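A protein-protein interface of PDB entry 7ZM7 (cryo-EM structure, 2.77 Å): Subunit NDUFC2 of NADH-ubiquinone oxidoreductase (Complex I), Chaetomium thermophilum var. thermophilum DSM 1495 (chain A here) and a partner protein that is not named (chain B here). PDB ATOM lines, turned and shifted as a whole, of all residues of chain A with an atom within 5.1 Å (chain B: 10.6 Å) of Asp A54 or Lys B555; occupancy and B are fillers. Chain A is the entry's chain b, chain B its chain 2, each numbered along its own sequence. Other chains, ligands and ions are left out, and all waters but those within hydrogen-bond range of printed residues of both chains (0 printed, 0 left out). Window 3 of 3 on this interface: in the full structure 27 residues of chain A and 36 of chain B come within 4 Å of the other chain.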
ATOM      1  N   ARG A   4     -32.399 -16.139  -5.026  1.00  0.00           N
ATOM      2  CA  ARG A   4     -32.723 -15.233  -6.153  1.00  0.00           C
ATOM      3  C   ARG A   4     -33.440 -16.049  -7.222  1.00  0.00           C
ATOM      4  O   ARG A   4     -34.421 -15.551  -7.788  1.00  0.00           O
ATOM      5  CB  ARG A   4     -31.431 -14.667  -6.745  1.00  0.00           C
ATOM      6  CG  ARG A   4     -31.425 -13.155  -6.909  1.00  0.00           C
ATOM      7  CD  ARG A   4     -30.117 -12.686  -7.512  1.00  0.00           C
ATOM      8  NE  ARG A   4     -28.964 -13.242  -6.820  1.00  0.00           N
ATOM      9  CZ  ARG A   4     -28.307 -12.638  -5.837  1.00  0.00           C
ATOM     10  NH1 ARG A   4     -27.271 -13.236  -5.276  1.00  0.00           N
ATOM     11  NH2 ARG A   4     -28.684 -11.445  -5.417  1.00  0.00           N
ATOM     12  N   LEU A  50     -28.793 -11.975 -12.567  1.00  0.00           N
ATOM     13  CA  LEU A  50     -28.640 -11.117 -11.362  1.00  0.00           C
ATOM     14  C   LEU A  50     -27.632 -11.714 -10.383  1.00  0.00           C
ATOM     15  O   LEU A  50     -27.119 -10.969  -9.550  1.00  0.00           O
ATOM     16  CB  LEU A  50     -30.012 -10.858 -10.731  1.00  0.00           C
ATOM     17  CG  LEU A  50     -30.873  -9.836 -11.466  1.00  0.00           C
ATOM     18  CD1 LEU A  50     -32.064  -9.439 -10.614  1.00  0.00           C
ATOM     19  CD2 LEU A  50     -30.059  -8.605 -11.829  1.00  0.00           C
ATOM     20  N   GLN A  51     -27.406 -13.019 -10.452  1.00  0.00           N
ATOM     21  CA  GLN A  51     -26.407 -13.688  -9.587  1.00  0.00           C
ATOM     22  C   GLN A  51     -25.023 -13.338 -10.122  1.00  0.00           C
ATOM     23  O   GLN A  51     -24.109 -13.149  -9.304  1.00  0.00           O
ATOM     24  CB  GLN A  51     -26.641 -15.196  -9.595  1.00  0.00           C
ATOM     25  CG  GLN A  51     -25.963 -15.934  -8.453  1.00  0.00           C
ATOM     26  CD  GLN A  51     -26.038 -17.425  -8.665  1.00  0.00           C
ATOM     27  OE1 GLN A  51     -26.438 -17.896  -9.726  1.00  0.00           O
ATOM     28  NE2 GLN A  51     -25.645 -18.179  -7.653  1.00  0.00           N
ATOM     29  N   SER A  52     -24.877 -13.274 -11.446  1.00  0.00           N
ATOM     30  CA  SER A  52     -23.603 -12.832 -11.991  1.00  0.00           C
ATOM     31  C   SER A  52     -23.364 -11.364 -11.694  1.00  0.00           C
ATOM     32  O   SER A  52     -22.227 -10.945 -11.468  1.00  0.00           O
ATOM     33  CB  SER A  52     -23.571 -13.085 -13.491  1.00  0.00           C
ATOM     34  OG  SER A  52     -24.797 -12.720 -14.081  1.00  0.00           O
ATOM     35  N   ILE A  53     -24.419 -10.561 -11.718  1.00  0.00           N
ATOM     36  CA  ILE A  53     -24.295  -9.165 -11.332  1.00  0.00           C
ATOM     37  C   ILE A  53     -23.888  -9.061  -9.874  1.00  0.00           C
ATOM     38  O   ILE A  53     -23.021  -8.260  -9.510  1.00  0.00           O
ATOM     39  CB  ILE A  53     -25.612  -8.422 -11.614  1.00  0.00           C
ATOM     40  CG1 ILE A  53     -25.985  -8.584 -13.081  1.00  0.00           C
ATOM     41  CG2 ILE A  53     -25.502  -6.963 -11.280  1.00  0.00           C
ATOM     42  CD1 ILE A  53     -25.003  -7.962 -14.021  1.00  0.00           C
ATOM     43  N   ASP A  54     -24.500  -9.868  -9.019  1.00  0.00           N
ATOM     44  CA  ASP A  54     -24.190  -9.801  -7.600  1.00  0.00           C
ATOM     45  C   ASP A  54     -22.744 -10.175  -7.338  1.00  0.00           C
ATOM     46  O   ASP A  54     -22.057  -9.530  -6.540  1.00  0.00           O
ATOM     47  CB  ASP A  54     -25.123 -10.712  -6.820  1.00  0.00           C
ATOM     48  CG  ASP A  54     -24.712 -10.847  -5.390  1.00  0.00           C
ATOM     49  OD1 ASP A  54     -24.513  -9.806  -4.741  1.00  0.00           O
ATOM     50  OD2 ASP A  54     -24.569 -11.991  -4.918  1.00  0.00           O
ATOM     51  N   GLU A  55     -22.267 -11.222  -8.006  1.00  0.00           N
ATOM     52  CA  GLU A  55     -20.920 -11.712  -7.768  1.00  0.00           C
ATOM     53  C   GLU A  55     -19.899 -10.629  -8.060  1.00  0.00           C
ATOM     54  O   GLU A  55     -18.982 -10.397  -7.265  1.00  0.00           O
ATOM     55  CB  GLU A  55     -20.676 -12.942  -8.639  1.00  0.00           C
ATOM     56  CG  GLU A  55     -19.337 -13.630  -8.491  1.00  0.00           C
ATOM     57  CD  GLU A  55     -19.137 -14.251  -7.121  1.00  0.00           C
ATOM     58  OE1 GLU A  55     -20.142 -14.589  -6.460  1.00  0.00           O
ATOM     59  OE2 GLU A  55     -17.970 -14.429  -6.716  1.00  0.00           O
ATOM     60  N   LYS A  56     -20.067  -9.928  -9.185  1.00  0.00           N
ATOM     61  CA  LYS A  56     -19.118  -8.903  -9.596  1.00  0.00           C
ATOM     62  C   LYS A  56     -19.181  -7.669  -8.705  1.00  0.00           C
ATOM     63  O   LYS A  56     -18.144  -7.100  -8.352  1.00  0.00           O
ATOM     64  CB  LYS A  56     -19.382  -8.542 -11.045  1.00  0.00           C
ATOM     65  CG  LYS A  56     -19.345  -9.749 -11.955  1.00  0.00           C
ATOM     66  CD  LYS A  56     -19.917  -9.444 -13.322  1.00  0.00           C
ATOM     67  CE  LYS A  56     -18.837  -8.926 -14.247  1.00  0.00           C
ATOM     68  NZ  LYS A  56     -17.851  -9.977 -14.612  1.00  0.00           N
ATOM     69  N   GLN A  57     -20.385  -7.237  -8.336  1.00  0.00           N
ATOM     70  CA  GLN A  57     -20.533  -6.089  -7.453  1.00  0.00           C
ATOM     71  C   GLN A  57     -19.864  -6.336  -6.114  1.00  0.00           C
ATOM     72  O   GLN A  57     -19.303  -5.417  -5.509  1.00  0.00           O
ATOM     73  CB  GLN A  57     -22.011  -5.787  -7.252  1.00  0.00           C
ATOM     74  CG  GLN A  57     -22.693  -5.230  -8.471  1.00  0.00           C
ATOM     75  CD  GLN A  57     -24.184  -5.189  -8.329  1.00  0.00           C
ATOM     76  OE1 GLN A  57     -24.874  -4.531  -9.097  1.00  0.00           O
ATOM     77  NE2 GLN A  57     -24.696  -5.907  -7.347  1.00  0.00           N
ATOM     78  N   THR A  58     -19.934  -7.575  -5.627  1.00  0.00           N
ATOM     79  CA  THR A  58     -19.303  -7.930  -4.362  1.00  0.00           C
ATOM     80  C   THR A  58     -17.790  -7.786  -4.433  1.00  0.00           C
ATOM     81  O   THR A  58     -17.158  -7.340  -3.475  1.00  0.00           O
ATOM     82  CB  THR A  58     -19.687  -9.356  -3.991  1.00  0.00           C
ATOM     83  OG1 THR A  58     -21.104  -9.500  -4.102  1.00  0.00           O
ATOM     84  CG2 THR A  58     -19.255  -9.675  -2.575  1.00  0.00           C
ATOM     85  N   PHE B 368     -31.170   6.493  -7.194  1.00  0.00           N
ATOM     86  CA  PHE B 368     -32.307   5.608  -7.005  1.00  0.00           C
ATOM     87  C   PHE B 368     -33.621   6.320  -7.291  1.00  0.00           C
ATOM     88  O   PHE B 368     -34.497   5.767  -7.959  1.00  0.00           O
ATOM     89  CB  PHE B 368     -32.299   5.045  -5.596  1.00  0.00           C
ATOM     90  CG  PHE B 368     -33.410   4.082  -5.337  1.00  0.00           C
ATOM     91  CD1 PHE B 368     -33.525   2.932  -6.078  1.00  0.00           C
ATOM     92  CD2 PHE B 368     -34.342   4.324  -4.361  1.00  0.00           C
ATOM     93  CE1 PHE B 368     -34.546   2.063  -5.852  1.00  0.00           C
ATOM     94  CE2 PHE B 368     -35.355   3.446  -4.140  1.00  0.00           C
ATOM     95  CZ  PHE B 368     -35.457   2.322  -4.885  1.00  0.00           C
ATOM     96  N   PHE B 449     -38.826   3.730  -0.109  1.00  0.00           N
ATOM     97  CA  PHE B 449     -37.395   3.563   0.011  1.00  0.00           C
ATOM     98  C   PHE B 449     -36.630   4.615  -0.762  1.00  0.00           C
ATOM     99  O   PHE B 449     -35.423   4.734  -0.585  1.00  0.00           O
ATOM    100  CB  PHE B 449     -37.001   2.173  -0.451  1.00  0.00           C
ATOM    101  CG  PHE B 449     -37.488   1.099   0.438  1.00  0.00           C
ATOM    102  CD1 PHE B 449     -36.912   0.898   1.680  1.00  0.00           C
ATOM    103  CD2 PHE B 449     -38.528   0.286   0.050  1.00  0.00           C
ATOM    104  CE1 PHE B 449     -37.353  -0.085   2.499  1.00  0.00           C
ATOM    105  CE2 PHE B 449     -38.966  -0.705   0.872  1.00  0.00           C
ATOM    106  CZ  PHE B 449     -38.376  -0.887   2.101  1.00  0.00           C
ATOM    107  N   MET B 453     -34.237   7.436   1.625  1.00  0.00           N
ATOM    108  CA  MET B 453     -32.816   7.716   1.311  1.00  0.00           C
ATOM    109  C   MET B 453     -32.565   9.215   1.161  1.00  0.00           C
ATOM    110  O   MET B 453     -31.552   9.677   1.665  1.00  0.00           O
ATOM    111  CB  MET B 453     -32.415   6.985   0.034  1.00  0.00           C
ATOM    112  CG  MET B 453     -32.389   5.479   0.172  1.00  0.00           C
ATOM    113  SD  MET B 453     -32.312   4.644  -1.431  1.00  0.00           S
ATOM    114  CE  MET B 453     -30.623   4.979  -1.922  1.00  0.00           C
ATOM    115  N   LEU B 549     -42.778  -5.640  -4.652  1.00  0.00           N
ATOM    116  CA  LEU B 549     -41.857  -6.701  -4.150  1.00  0.00           C
ATOM    117  C   LEU B 549     -40.397  -6.255  -4.067  1.00  0.00           C
ATOM    118  O   LEU B 549     -39.560  -7.135  -3.922  1.00  0.00           O
ATOM    119  CB  LEU B 549     -41.994  -7.930  -5.056  1.00  0.00           C
ATOM    120  CG  LEU B 549     -43.372  -8.587  -5.095  1.00  0.00           C
ATOM    121  CD1 LEU B 549     -43.420  -9.683  -6.145  1.00  0.00           C
ATOM    122  CD2 LEU B 549     -43.750  -9.139  -3.732  1.00  0.00           C
ATOM    123  N   PHE B 550     -40.121  -4.950  -4.037  1.00  0.00           N
ATOM    124  CA  PHE B 550     -38.739  -4.397  -4.011  1.00  0.00           C
ATOM    125  C   PHE B 550     -37.976  -4.848  -2.764  1.00  0.00           C
ATOM    126  O   PHE B 550     -36.772  -5.098  -2.879  1.00  0.00           O
ATOM    127  CB  PHE B 550     -38.790  -2.870  -4.093  1.00  0.00           C
ATOM    128  CG  PHE B 550     -37.472  -2.158  -3.926  1.00  0.00           C
ATOM    129  CD1 PHE B 550     -36.574  -2.075  -4.976  1.00  0.00           C
ATOM    130  CD2 PHE B 550     -37.138  -1.561  -2.722  1.00  0.00           C
ATOM    131  CE1 PHE B 550     -35.364  -1.420  -4.819  1.00  0.00           C
ATOM    132  CE2 PHE B 550     -35.929  -0.907  -2.567  1.00  0.00           C
ATOM    133  CZ  PHE B 550     -35.046  -0.836  -3.617  1.00  0.00           C
ATOM    134  N   ILE B 551     -38.649  -4.971  -1.622  1.00  0.00           N
ATOM    135  CA  ILE B 551     -37.975  -5.313  -0.339  1.00  0.00           C
ATOM    136  C   ILE B 551     -37.339  -6.705  -0.423  1.00  0.00           C
ATOM    137  O   ILE B 551     -36.512  -7.019   0.443  1.00  0.00           O
ATOM    138  CB  ILE B 551     -38.960  -5.149   0.833  1.00  0.00           C
ATOM    139  CG1 ILE B 551     -38.240  -4.814   2.142  1.00  0.00           C
ATOM    140  CG2 ILE B 551     -39.875  -6.350   0.977  1.00  0.00           C
ATOM    141  CD1 ILE B 551     -39.164  -4.492   3.286  1.00  0.00           C
ATOM    142  N   PHE B 552     -37.750  -7.529  -1.386  1.00  0.00           N
ATOM    143  CA  PHE B 552     -37.191  -8.887  -1.577  1.00  0.00           C
ATOM    144  C   PHE B 552     -36.204  -8.921  -2.752  1.00  0.00           C
ATOM    145  O   PHE B 552     -35.676 -10.004  -3.024  1.00  0.00           O
ATOM    146  CB  PHE B 552     -38.341  -9.873  -1.793  1.00  0.00           C
ATOM    147  CG  PHE B 552     -39.407  -9.839  -0.732  1.00  0.00           C
ATOM    148  CD1 PHE B 552     -40.651  -9.291  -0.993  1.00  0.00           C
ATOM    149  CD2 PHE B 552     -39.165 -10.347   0.532  1.00  0.00           C
ATOM    150  CE1 PHE B 552     -41.630  -9.258  -0.014  1.00  0.00           C
ATOM    151  CE2 PHE B 552     -40.143 -10.313   1.512  1.00  0.00           C
ATOM    152  CZ  PHE B 552     -41.373  -9.768   1.237  1.00  0.00           C
ATOM    153  N   MET B 553     -35.963  -7.794  -3.430  1.00  0.00           N
ATOM    154  CA  MET B 553     -35.127  -7.798  -4.666  1.00  0.00           C
ATOM    155  C   MET B 553     -34.373  -6.482  -4.774  1.00  0.00           C
ATOM    156  O   MET B 553     -34.311  -5.931  -5.877  1.00  0.00           O
ATOM    157  CB  MET B 553     -35.997  -7.930  -5.916  1.00  0.00           C
ATOM    158  CG  MET B 553     -37.265  -7.126  -5.859  1.00  0.00           C
ATOM    159  SD  MET B 553     -37.940  -6.693  -7.472  1.00  0.00           S
ATOM    160  CE  MET B 553     -36.983  -5.223  -7.821  1.00  0.00           C
ATOM    161  N   ASN B 554     -33.773  -6.042  -3.680  1.00  0.00           N
ATOM    162  CA  ASN B 554     -33.115  -4.711  -3.624  1.00  0.00           C
ATOM    163  C   ASN B 554     -31.589  -4.736  -3.792  1.00  0.00           C
ATOM    164  O   ASN B 554     -31.052  -3.665  -4.084  1.00  0.00           O
ATOM    165  CB  ASN B 554     -33.596  -3.942  -2.384  1.00  0.00           C
ATOM    166  CG  ASN B 554     -33.387  -4.678  -1.079  1.00  0.00           C
ATOM    167  OD1 ASN B 554     -32.346  -4.543  -0.446  1.00  0.00           O
ATOM    168  ND2 ASN B 554     -34.379  -5.443  -0.659  1.00  0.00           N
ATOM    169  N   LYS B 555     -30.917  -5.881  -3.682  1.00  0.00           N
ATOM    170  CA  LYS B 555     -29.423  -5.829  -3.692  1.00  0.00           C
ATOM    171  C   LYS B 555     -28.781  -5.321  -4.995  1.00  0.00           C
ATOM    172  O   LYS B 555     -27.984  -4.404  -4.896  1.00  0.00           O
ATOM    173  CB  LYS B 555     -28.771  -7.112  -3.175  1.00  0.00           C
ATOM    174  CG  LYS B 555     -27.397  -6.910  -2.557  1.00  0.00           C
ATOM    175  CD  LYS B 555     -26.670  -8.193  -2.242  1.00  0.00           C
ATOM    176  CE  LYS B 555     -25.266  -7.939  -1.740  1.00  0.00           C
ATOM    177  NZ  LYS B 555     -25.250  -6.918  -0.667  1.00  0.00           N
ATOM    178  N   GLU B 556     -29.162  -5.811  -6.170  1.00  0.00           N
ATOM    179  CA  GLU B 556     -28.462  -5.402  -7.420  1.00  0.00           C
ATOM    180  C   GLU B 556     -28.724  -3.940  -7.781  1.00  0.00           C
ATOM    181  O   GLU B 556     -27.772  -3.279  -8.203  1.00  0.00           O
ATOM    182  CB  GLU B 556     -28.748  -6.372  -8.563  1.00  0.00           C
ATOM    183  CG  GLU B 556     -27.974  -7.671  -8.466  1.00  0.00           C
ATOM    184  CD  GLU B 556     -28.363  -8.573  -7.309  1.00  0.00           C
ATOM    185  OE1 GLU B 556     -29.384  -9.275  -7.424  1.00  0.00           O
ATOM    186  OE2 GLU B 556     -27.649  -8.566  -6.296  1.00  0.00           O
ATOM    187  N   TRP B 557     -29.957  -3.467  -7.622  1.00  0.00           N
ATOM    188  CA  TRP B 557     -30.349  -2.079  -7.977  1.00  0.00           C
ATOM    189  C   TRP B 557     -29.613  -1.073  -7.083  1.00  0.00           C
ATOM    190  O   TRP B 557     -29.008  -0.138  -7.629  1.00  0.00           O
ATOM    191  CB  TRP B 557     -31.880  -1.959  -7.936  1.00  0.00           C
ATOM    192  CG  TRP B 557     -32.527  -0.726  -8.486  1.00  0.00           C
ATOM    193  CD1 TRP B 557     -31.933   0.416  -8.933  1.00  0.00           C
ATOM    194  CD2 TRP B 557     -33.942  -0.521  -8.634  1.00  0.00           C
ATOM    195  NE1 TRP B 557     -32.879   1.314  -9.347  1.00  0.00           N
ATOM    196  CE2 TRP B 557     -34.121   0.764  -9.180  1.00  0.00           C
ATOM    197  CE3 TRP B 557     -35.072  -1.302  -8.366  1.00  0.00           C
ATOM    198  CZ2 TRP B 557     -35.383   1.284  -9.454  1.00  0.00           C
ATOM    199  CZ3 TRP B 557     -36.318  -0.790  -8.639  1.00  0.00           C
ATOM    200  CH2 TRP B 557     -36.469   0.488  -9.177  1.00  0.00           C
ATOM    201  N   LEU B 558     -29.655  -1.261  -5.765  1.00  0.00           N
ATOM    202  CA  LEU B 558     -29.008  -0.297  -4.839  1.00  0.00           C
ATOM    203  C   LEU B 558     -27.482  -0.404  -4.910  1.00  0.00           C
ATOM    204  O   LEU B 558     -26.827   0.640  -4.799  1.00  0.00           O
ATOM    205  CB  LEU B 558     -29.580  -0.472  -3.431  1.00  0.00           C
ATOM    206  CG  LEU B 558     -31.059  -0.122  -3.289  1.00  0.00           C
ATOM    207  CD1 LEU B 558     -31.600  -0.568  -1.940  1.00  0.00           C
ATOM    208  CD2 LEU B 558     -31.279   1.369  -3.489  1.00  0.00           C
ATOM    209  N   SER B 559     -26.947  -1.615  -5.069  1.00  0.00           N
ATOM    210  CA  SER B 559     -25.476  -1.840  -5.176  1.00  0.00           C
ATOM    211  C   SER B 559     -24.906  -1.156  -6.418  1.00  0.00           C
ATOM    212  O   SER B 559     -23.785  -0.667  -6.343  1.00  0.00           O
ATOM    213  CB  SER B 559     -25.133  -3.299  -5.143  1.00  0.00           C
ATOM    214  OG  SER B 559     -25.247  -3.818  -3.828  1.00  0.00           O
ATOM    215  N   MET B 560     -25.655  -1.132  -7.518  1.00  0.00           N
ATOM    216  CA  MET B 560     -25.209  -0.454  -8.754  1.00  0.00           C
ATOM    217  C   MET B 560     -24.997   1.016  -8.430  1.00  0.00           C
ATOM    218  O   MET B 560     -23.977   1.560  -8.845  1.00  0.00           O
ATOM    219  CB  MET B 560     -26.338  -0.550  -9.783  1.00  0.00           C
ATOM    220  CG  MET B 560     -26.093   0.211 -11.063  1.00  0.00           C
ATOM    221  SD  MET B 560     -27.637   0.378 -11.980  1.00  0.00           S
ATOM    222  CE  MET B 560     -28.254   1.913 -11.296  1.00  0.00           C
ATOM    223  N   GLY B 561     -25.926   1.616  -7.690  1.00  0.00           N
ATOM    224  CA  GLY B 561     -25.805   3.030  -7.303  1.00  0.00           C
ATOM    225  C   GLY B 561     -24.645   3.271  -6.359  1.00  0.00           C
ATOM    226  O   GLY B 561     -23.961   4.286  -6.534  1.00  0.00           O
ATOM    227  N   THR B 562     -24.436   2.376  -5.394  1.00  0.00           N
ATOM    228  CA  THR B 562     -23.320   2.533  -4.426  1.00  0.00           C
ATOM    229  C   THR B 562     -21.983   2.478  -5.167  1.00  0.00           C
ATOM    230  O   THR B 562     -21.129   3.309  -4.847  1.00  0.00           O
ATOM    231  CB  THR B 562     -23.461   1.629  -3.192  1.00  0.00           C
ATOM    232  OG1 THR B 562     -22.696   2.216  -2.140  1.00  0.00           O
ATOM    233  CG2 THR B 562     -23.001   0.204  -3.404  1.00  0.00           C
ATOM    234  N   ILE B 563     -21.838   1.579  -6.146  1.00  0.00           N
ATOM    235  CA  ILE B 563     -20.591   1.498  -6.961  1.00  0.00           C
ATOM    236  C   ILE B 563     -20.489   2.748  -7.837  1.00  0.00           C
ATOM    237  O   ILE B 563     -19.380   3.298  -7.946  1.00  0.00           O
ATOM    238  CB  ILE B 563     -20.555   0.213  -7.803  1.00  0.00           C
ATOM    239  CG1 ILE B 563     -20.707  -1.039  -6.939  1.00  0.00           C
ATOM    240  CG2 ILE B 563     -19.296   0.149  -8.652  1.00  0.00           C
ATOM    241  CD1 ILE B 563     -20.580  -2.325  -7.709  1.00  0.00           C
ATOM    242  N   LEU B 564     -21.597   3.191  -8.428  1.00  0.00           N
ATOM    243  CA  LEU B 564     -21.493   4.335  -9.324  1.00  0.00           C
ATOM    244  C   LEU B 564     -21.041   5.576  -8.581  1.00  0.00           C
ATOM    245  O   LEU B 564     -20.184   6.320  -9.065  1.00  0.00           O
ATOM    246  CB  LEU B 564     -22.821   4.597 -10.024  1.00  0.00           C
ATOM    247  CG  LEU B 564     -23.194   3.652 -11.150  1.00  0.00           C
ATOM    248  CD1 LEU B 564     -24.531   4.021 -11.706  1.00  0.00           C
ATOM    249  CD2 LEU B 564     -22.151   3.697 -12.205  1.00  0.00           C
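The side-chain carboxylate (OE1) of Glu B556 lies within salt-bridge range of the guanidinium group (NH2) of Arg A4.
O of Glu B556 sits close to OE1 of Gln A57 (3.3 Å).
The backbone carbonyl oxygen (O) of Lys B555 lies within hydrogen-bond range of the side-chain hydroxyl (OG) of Ser B559, 3.0 Å away.
The guanidinium group (NH1) of Arg A4 lies within salt-bridge range of the side-chain carboxylate (OD2) of Asp A54 (3.0 Å).
O of Asp A54 is in hydrogen-bond range of OG1 of Thr A58, 2.6 Å away.
Of the printed residues of chain B, Arg A4 touches Glu B556 (3.0 Å).
No residue of chain B comes within 4 Å of Ser A52.
Ile A53 touches just one residue of chain B: Glu B556 (3.8 Å).
Asp A54 touches just these residues of chain B: Lys B555 (3.6 Å) and Glu B556 (3.4 Å).
No residue of chain B comes within 4 Å of Thr A58.
Leu B549 touches none of the printed residues of chain A.
Lys B555 touches just one residue of chain A: Asp A54 (3.6 Å).
Trp B557 touches none of the printed residues of chain A.
Of the printed residues of chain A, Met B560 touches Gln A57 (3.8 Å).
The nearest residue of chain B that does not touch Asp A54 is Ser B559 (6.1 Å).
The nearest printed residue of chain A that does not touch Glu B556 is Gln A51 (5.2 Å).
Among the printed residues, merely in contact across the chains: Leu A50 with Glu B556, Ile A53 with Glu B556, Asp A54 with Lys B555, Asp A54 with Glu B556, Gln A57 with Ser B559, Gln A57 with Met B560 and Gln A57 with Ile B563.
Printed residues of chain B that touch a printed residue of chain A: Lys B555, Glu B556, Ser B559, Met B560 and Ile B563.
Hydrophobic or aromatic side chains of chain B within 4 Å of the printed part of chain A: Ile B563.
Along chain B the printed residues that touch a printed residue of chain A span positions 555 to 563.
Hydrophobic or aromatic side chains of chain A within 4 Å of the printed part of chain B: Leu A50 and Ile A53.
Among the printed residues, 9 pairs touch across the chains.
Among the printed residues, Asp or Glu carboxylates within 4 Å of a Lys or Arg side-chain nitrogen of the other chain: Arg A4 with Glu B556 (3.0 Å).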
